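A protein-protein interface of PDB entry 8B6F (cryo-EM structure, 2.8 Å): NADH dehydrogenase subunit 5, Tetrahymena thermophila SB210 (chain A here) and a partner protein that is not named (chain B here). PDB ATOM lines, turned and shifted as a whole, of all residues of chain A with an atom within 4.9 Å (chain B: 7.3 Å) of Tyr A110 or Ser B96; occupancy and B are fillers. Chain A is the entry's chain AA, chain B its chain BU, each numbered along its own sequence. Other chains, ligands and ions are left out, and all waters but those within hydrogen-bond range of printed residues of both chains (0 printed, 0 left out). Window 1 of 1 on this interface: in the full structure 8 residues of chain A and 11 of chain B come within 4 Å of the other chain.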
ATOM      1  N   THR A 105      16.836  23.344  12.599  1.00  0.00           N
ATOM      2  CA  THR A 105      17.688  22.691  13.586  1.00  0.00           C
ATOM      3  C   THR A 105      17.610  21.176  13.465  1.00  0.00           C
ATOM      4  O   THR A 105      18.627  20.484  13.588  1.00  0.00           O
ATOM      5  CB  THR A 105      17.301  23.133  14.998  1.00  0.00           C
ATOM      6  OG1 THR A 105      15.890  22.975  15.186  1.00  0.00           O
ATOM      7  CG2 THR A 105      17.688  24.586  15.228  1.00  0.00           C
ATOM      8  N   TRP A 106      16.411  20.637  13.235  1.00  0.00           N
ATOM      9  CA  TRP A 106      16.278  19.194  13.058  1.00  0.00           C
ATOM     10  C   TRP A 106      17.092  18.715  11.864  1.00  0.00           C
ATOM     11  O   TRP A 106      17.828  17.727  11.956  1.00  0.00           O
ATOM     12  CB  TRP A 106      14.802  18.828  12.883  1.00  0.00           C
ATOM     13  CG  TRP A 106      14.575  17.414  12.436  1.00  0.00           C
ATOM     14  CD1 TRP A 106      14.598  16.945  11.154  1.00  0.00           C
ATOM     15  CD2 TRP A 106      14.285  16.285  13.269  1.00  0.00           C
ATOM     16  NE1 TRP A 106      14.342  15.597  11.139  1.00  0.00           N
ATOM     17  CE2 TRP A 106      14.147  15.167  12.425  1.00  0.00           C
ATOM     18  CE3 TRP A 106      14.130  16.113  14.647  1.00  0.00           C
ATOM     19  CZ2 TRP A 106      13.863  13.894  12.913  1.00  0.00           C
ATOM     20  CZ3 TRP A 106      13.848  14.848  15.131  1.00  0.00           C
ATOM     21  CH2 TRP A 106      13.719  13.755  14.266  1.00  0.00           C
ATOM     22  N   TYR A 107      16.969  19.401  10.729  1.00  0.00           N
ATOM     23  CA  TYR A 107      17.704  18.984   9.541  1.00  0.00           C
ATOM     24  C   TYR A 107      19.207  19.140   9.744  1.00  0.00           C
ATOM     25  O   TYR A 107      19.991  18.295   9.297  1.00  0.00           O
ATOM     26  CB  TYR A 107      17.230  19.773   8.323  1.00  0.00           C
ATOM     27  CG  TYR A 107      17.613  19.129   7.013  1.00  0.00           C
ATOM     28  CD1 TYR A 107      17.074  17.905   6.637  1.00  0.00           C
ATOM     29  CD2 TYR A 107      18.504  19.746   6.148  1.00  0.00           C
ATOM     30  CE1 TYR A 107      17.419  17.310   5.439  1.00  0.00           C
ATOM     31  CE2 TYR A 107      18.852  19.160   4.946  1.00  0.00           C
ATOM     32  CZ  TYR A 107      18.309  17.943   4.598  1.00  0.00           C
ATOM     33  OH  TYR A 107      18.659  17.361   3.403  1.00  0.00           O
ATOM     34  N   TYR A 108      19.623  20.211  10.421  1.00  0.00           N
ATOM     35  CA  TYR A 108      21.044  20.420  10.680  1.00  0.00           C
ATOM     36  C   TYR A 108      21.602  19.325  11.578  1.00  0.00           C
ATOM     37  O   TYR A 108      22.694  18.805  11.329  1.00  0.00           O
ATOM     38  CB  TYR A 108      21.260  21.799  11.303  1.00  0.00           C
ATOM     39  CG  TYR A 108      22.694  22.096  11.673  1.00  0.00           C
ATOM     40  CD1 TYR A 108      23.634  22.416  10.702  1.00  0.00           C
ATOM     41  CD2 TYR A 108      23.102  22.076  12.999  1.00  0.00           C
ATOM     42  CE1 TYR A 108      24.943  22.694  11.040  1.00  0.00           C
ATOM     43  CE2 TYR A 108      24.406  22.352  13.347  1.00  0.00           C
ATOM     44  CZ  TYR A 108      25.323  22.662  12.366  1.00  0.00           C
ATOM     45  OH  TYR A 108      26.624  22.938  12.714  1.00  0.00           O
ATOM     46  N   ASN A 109      20.859  18.951  12.621  1.00  0.00           N
ATOM     47  CA  ASN A 109      21.306  17.872  13.494  1.00  0.00           C
ATOM     48  C   ASN A 109      21.385  16.555  12.733  1.00  0.00           C
ATOM     49  O   ASN A 109      22.316  15.768  12.935  1.00  0.00           O
ATOM     50  CB  ASN A 109      20.375  17.747  14.698  1.00  0.00           C
ATOM     51  CG  ASN A 109      20.337  19.009  15.536  1.00  0.00           C
ATOM     52  OD1 ASN A 109      21.295  19.782  15.556  1.00  0.00           O
ATOM     53  ND2 ASN A 109      19.230  19.223  16.234  1.00  0.00           N
ATOM     54  N   TYR A 110      20.411  16.292  11.861  1.00  0.00           N
ATOM     55  CA  TYR A 110      20.470  15.090  11.038  1.00  0.00           C
ATOM     56  C   TYR A 110      21.705  15.097  10.148  1.00  0.00           C
ATOM     57  O   TYR A 110      22.381  14.072  10.007  1.00  0.00           O
ATOM     58  CB  TYR A 110      19.207  14.963  10.186  1.00  0.00           C
ATOM     59  CG  TYR A 110      19.414  14.085   8.975  1.00  0.00           C
ATOM     60  CD1 TYR A 110      19.523  12.706   9.100  1.00  0.00           C
ATOM     61  CD2 TYR A 110      19.520  14.639   7.705  1.00  0.00           C
ATOM     62  CE1 TYR A 110      19.721  11.902   7.993  1.00  0.00           C
ATOM     63  CE2 TYR A 110      19.718  13.845   6.595  1.00  0.00           C
ATOM     64  CZ  TYR A 110      19.817  12.479   6.745  1.00  0.00           C
ATOM     65  OH  TYR A 110      20.017  11.689   5.638  1.00  0.00           O
ATOM     66  N   ILE A 111      22.016  16.241   9.537  1.00  0.00           N
ATOM     67  CA  ILE A 111      23.190  16.318   8.675  1.00  0.00           C
ATOM     68  C   ILE A 111      24.456  16.056   9.477  1.00  0.00           C
ATOM     69  O   ILE A 111      25.340  15.310   9.040  1.00  0.00           O
ATOM     70  CB  ILE A 111      23.251  17.683   7.965  1.00  0.00           C
ATOM     71  CG1 ILE A 111      22.140  17.803   6.925  1.00  0.00           C
ATOM     72  CG2 ILE A 111      24.606  17.892   7.292  1.00  0.00           C
ATOM     73  CD1 ILE A 111      21.943  19.214   6.433  1.00  0.00           C
ATOM     74  N   LEU A 112      24.566  16.655  10.662  1.00  0.00           N
ATOM     75  CA  LEU A 112      25.759  16.442  11.473  1.00  0.00           C
ATOM     76  C   LEU A 112      25.898  14.981  11.872  1.00  0.00           C
ATOM     77  O   LEU A 112      26.998  14.418  11.817  1.00  0.00           O
ATOM     78  CB  LEU A 112      25.721  17.327  12.717  1.00  0.00           C
ATOM     79  CG  LEU A 112      25.792  18.843  12.516  1.00  0.00           C
ATOM     80  CD1 LEU A 112      26.156  19.512  13.830  1.00  0.00           C
ATOM     81  CD2 LEU A 112      26.745  19.231  11.407  1.00  0.00           C
ATOM     82  N   ASN A 113      24.802  14.349  12.287  1.00  0.00           N
ATOM     83  CA  ASN A 113      24.867  12.936  12.635  1.00  0.00           C
ATOM     84  C   ASN A 113      25.256  12.099  11.426  1.00  0.00           C
ATOM     85  O   ASN A 113      26.063  11.169  11.536  1.00  0.00           O
ATOM     86  CB  ASN A 113      23.525  12.472  13.197  1.00  0.00           C
ATOM     87  CG  ASN A 113      23.157  13.179  14.480  1.00  0.00           C
ATOM     88  OD1 ASN A 113      23.758  14.191  14.839  1.00  0.00           O
ATOM     89  ND2 ASN A 113      22.160  12.654  15.178  1.00  0.00           N
ATOM     90  N   PHE A 114      24.686  12.413  10.261  1.00  0.00           N
ATOM     91  CA  PHE A 114      25.019  11.669   9.052  1.00  0.00           C
ATOM     92  C   PHE A 114      26.499  11.795   8.720  1.00  0.00           C
ATOM     93  O   PHE A 114      27.150  10.805   8.367  1.00  0.00           O
ATOM     94  CB  PHE A 114      24.161  12.172   7.888  1.00  0.00           C
ATOM     95  CG  PHE A 114      24.513  11.559   6.562  1.00  0.00           C
ATOM     96  CD1 PHE A 114      25.450  12.154   5.734  1.00  0.00           C
ATOM     97  CD2 PHE A 114      23.892  10.398   6.136  1.00  0.00           C
ATOM     98  CE1 PHE A 114      25.770  11.594   4.512  1.00  0.00           C
ATOM     99  CE2 PHE A 114      24.207   9.833   4.914  1.00  0.00           C
ATOM    100  CZ  PHE A 114      25.148  10.432   4.102  1.00  0.00           C
ATOM    101  N   LEU A 121      20.193  13.553  18.154  1.00  0.00           N
ATOM    102  CA  LEU A 121      19.834  14.963  18.298  1.00  0.00           C
ATOM    103  C   LEU A 121      19.714  15.283  19.788  1.00  0.00           C
ATOM    104  O   LEU A 121      18.634  15.522  20.330  1.00  0.00           O
ATOM    105  CB  LEU A 121      18.542  15.273  17.552  1.00  0.00           C
ATOM    106  CG  LEU A 121      18.500  15.013  16.040  1.00  0.00           C
ATOM    107  CD1 LEU A 121      18.311  13.535  15.701  1.00  0.00           C
ATOM    108  CD2 LEU A 121      17.409  15.847  15.393  1.00  0.00           C
ATOM    109  N   GLN B  58      24.361   4.805   6.027  1.00  0.00           N
ATOM    110  CA  GLN B  58      24.765   5.918   5.175  1.00  0.00           C
ATOM    111  C   GLN B  58      24.899   5.464   3.730  1.00  0.00           C
ATOM    112  O   GLN B  58      24.496   6.177   2.804  1.00  0.00           O
ATOM    113  CB  GLN B  58      26.087   6.512   5.665  1.00  0.00           C
ATOM    114  CG  GLN B  58      26.178   6.721   7.169  1.00  0.00           C
ATOM    115  CD  GLN B  58      25.175   7.728   7.682  1.00  0.00           C
ATOM    116  OE1 GLN B  58      25.536   8.852   8.021  1.00  0.00           O
ATOM    117  NE2 GLN B  58      23.908   7.331   7.750  1.00  0.00           N
ATOM    118  N   GLN B  61      21.464   5.092   2.201  1.00  0.00           N
ATOM    119  CA  GLN B  61      20.872   6.407   1.970  1.00  0.00           C
ATOM    120  C   GLN B  61      21.434   7.035   0.703  1.00  0.00           C
ATOM    121  O   GLN B  61      20.681   7.516  -0.153  1.00  0.00           O
ATOM    122  CB  GLN B  61      21.118   7.316   3.173  1.00  0.00           C
ATOM    123  CG  GLN B  61      20.274   6.977   4.389  1.00  0.00           C
ATOM    124  CD  GLN B  61      20.603   7.847   5.585  1.00  0.00           C
ATOM    125  OE1 GLN B  61      21.759   7.948   5.995  1.00  0.00           O
ATOM    126  NE2 GLN B  61      19.586   8.485   6.150  1.00  0.00           N
ATOM    127  N   ALA B  90      11.905  16.023  -1.022  1.00  0.00           N
ATOM    128  CA  ALA B  90      11.111  15.115  -0.203  1.00  0.00           C
ATOM    129  C   ALA B  90      11.931  13.908   0.230  1.00  0.00           C
ATOM    130  O   ALA B  90      11.856  13.478   1.387  1.00  0.00           O
ATOM    131  CB  ALA B  90       9.867  14.669  -0.971  1.00  0.00           C
ATOM    132  N   LEU B  91      12.723  13.347  -0.686  1.00  0.00           N
ATOM    133  CA  LEU B  91      13.564  12.209  -0.333  1.00  0.00           C
ATOM    134  C   LEU B  91      14.596  12.597   0.717  1.00  0.00           C
ATOM    135  O   LEU B  91      14.820  11.858   1.682  1.00  0.00           O
ATOM    136  CB  LEU B  91      14.245  11.661  -1.586  1.00  0.00           C
ATOM    137  CG  LEU B  91      15.117  10.419  -1.395  1.00  0.00           C
ATOM    138  CD1 LEU B  91      14.293   9.250  -0.881  1.00  0.00           C
ATOM    139  CD2 LEU B  91      15.810  10.055  -2.694  1.00  0.00           C
ATOM    140  N   LEU B  92      15.236  13.756   0.547  1.00  0.00           N
ATOM    141  CA  LEU B  92      16.223  14.206   1.524  1.00  0.00           C
ATOM    142  C   LEU B  92      15.579  14.404   2.890  1.00  0.00           C
ATOM    143  O   LEU B  92      16.153  14.028   3.918  1.00  0.00           O
ATOM    144  CB  LEU B  92      16.883  15.499   1.046  1.00  0.00           C
ATOM    145  CG  LEU B  92      17.772  15.385  -0.193  1.00  0.00           C
ATOM    146  CD1 LEU B  92      18.226  16.758  -0.649  1.00  0.00           C
ATOM    147  CD2 LEU B  92      18.973  14.493   0.076  1.00  0.00           C
ATOM    148  N   GLY B  93      14.386  14.997   2.919  1.00  0.00           N
ATOM    149  CA  GLY B  93      13.693  15.190   4.180  1.00  0.00           C
ATOM    150  C   GLY B  93      13.275  13.879   4.818  1.00  0.00           C
ATOM    151  O   GLY B  93      13.349  13.720   6.040  1.00  0.00           O
ATOM    152  N   SER B  94      12.825  12.922   4.004  1.00  0.00           N
ATOM    153  CA  SER B  94      12.441  11.621   4.541  1.00  0.00           C
ATOM    154  C   SER B  94      13.636  10.892   5.141  1.00  0.00           C
ATOM    155  O   SER B  94      13.499  10.187   6.148  1.00  0.00           O
ATOM    156  CB  SER B  94      11.796  10.771   3.447  1.00  0.00           C
ATOM    157  OG  SER B  94      10.626  11.392   2.943  1.00  0.00           O
ATOM    158  N   PHE B  95      14.817  11.041   4.537  1.00  0.00           N
ATOM    159  CA  PHE B  95      16.015  10.459   5.135  1.00  0.00           C
ATOM    160  C   PHE B  95      16.201  10.929   6.571  1.00  0.00           C
ATOM    161  O   PHE B  95      16.692  10.170   7.412  1.00  0.00           O
ATOM    162  CB  PHE B  95      17.252  10.813   4.304  1.00  0.00           C
ATOM    163  CG  PHE B  95      17.346  10.084   2.986  1.00  0.00           C
ATOM    164  CD1 PHE B  95      16.745   8.847   2.799  1.00  0.00           C
ATOM    165  CD2 PHE B  95      18.059  10.639   1.934  1.00  0.00           C
ATOM    166  CE1 PHE B  95      16.845   8.187   1.590  1.00  0.00           C
ATOM    167  CE2 PHE B  95      18.161   9.983   0.723  1.00  0.00           C
ATOM    168  CZ  PHE B  95      17.553   8.756   0.551  1.00  0.00           C
ATOM    169  N   SER B  96      15.816  12.170   6.866  1.00  0.00           N
ATOM    170  CA  SER B  96      15.975  12.706   8.213  1.00  0.00           C
ATOM    171  C   SER B  96      14.945  12.145   9.185  1.00  0.00           C
ATOM    172  O   SER B  96      15.214  12.073  10.389  1.00  0.00           O
ATOM    173  CB  SER B  96      15.881  14.233   8.181  1.00  0.00           C
ATOM    174  OG  SER B  96      14.628  14.657   7.679  1.00  0.00           O
ATOM    175  N   LEU B  97      13.770  11.750   8.694  1.00  0.00           N
ATOM    176  CA  LEU B  97      12.720  11.234   9.566  1.00  0.00           C
ATOM    177  C   LEU B  97      12.996   9.823  10.062  1.00  0.00           C
ATOM    178  O   LEU B  97      12.277   9.349  10.947  1.00  0.00           O
ATOM    179  CB  LEU B  97      11.372  11.267   8.844  1.00  0.00           C
ATOM    180  CG  LEU B  97      10.924  12.631   8.314  1.00  0.00           C
ATOM    181  CD1 LEU B  97       9.562  12.525   7.651  1.00  0.00           C
ATOM    182  CD2 LEU B  97      10.896  13.674   9.424  1.00  0.00           C
ATOM    183  N   LEU B  98      14.006   9.142   9.525  1.00  0.00           N
ATOM    184  CA  LEU B  98      14.365   7.799   9.979  1.00  0.00           C
ATOM    185  C   LEU B  98      15.294   7.945  11.176  1.00  0.00           C
ATOM    186  O   LEU B  98      16.507   8.115  11.025  1.00  0.00           O
ATOM    187  CB  LEU B  98      15.017   7.007   8.851  1.00  0.00           C
ATOM    188  CG  LEU B  98      14.178   6.877   7.577  1.00  0.00           C
ATOM    189  CD1 LEU B  98      14.988   6.248   6.454  1.00  0.00           C
ATOM    190  CD2 LEU B  98      12.918   6.069   7.846  1.00  0.00           C
ATOM    191  N   ASN B  99      14.717   7.874  12.375  1.00  0.00           N
ATOM    192  CA  ASN B  99      15.436   8.063  13.634  1.00  0.00           C
ATOM    193  C   ASN B  99      15.202   6.854  14.529  1.00  0.00           C
ATOM    194  O   ASN B  99      14.333   6.883  15.411  1.00  0.00           O
ATOM    195  CB  ASN B  99      14.987   9.349  14.329  1.00  0.00           C
ATOM    196  CG  ASN B  99      15.755   9.621  15.607  1.00  0.00           C
ATOM    197  OD1 ASN B  99      16.892   9.179  15.768  1.00  0.00           O
ATOM    198  ND2 ASN B  99      15.131  10.344  16.528  1.00  0.00           N
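OH of Tyr A110 sits at hydrogen-bond distance from NE2 of Gln B61, 3.3 Å away.
O of Phe A114 lies close to OE1 of Gln B58.
OE1 of Gln B61 lies within hydrogen-bond range of NE2 of Gln B58 (2.8 Å).
O of Ser B96 touches CZ2 of Trp A106 (3.4 Å).
Tyr A107 touches Leu B92 (OH to CB, 3.5 Å).
Tyr A110 touches Phe B95.
Tyr A110 touches Ser B96.
Phe A114 touches Gln B61.
Tyr A110 touches just these residues of chain B: Gln B61 (3.3 Å), Phe B95 (3.2 Å) and Ser B96 (3.6 Å).
Of chain A, only Trp A106 and Tyr A110 come within 4 Å of Ser B96.
Printed residues of chain B within 4 Å of Phe A114: Gln B58 and Gln B61.
Of the printed residues of chain A, Leu B92 touches Tyr A107.
Printed residues of chain A within 4 Å of Gln B61: Tyr A110 and Phe A114.
The nearest residue of chain A that does not touch Ser B96 is Tyr A107 (4.2 Å).
The nearest printed residue of chain B that does not touch Tyr A107 is Ser B96 (4.2 Å).
Of the 12 printed residues of chain B, 5 touch a printed residue of chain A.
Among the printed residues, no Asp or Glu carboxylate lies within 4 Å of a Lys or Arg side-chain nitrogen of the other chain.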
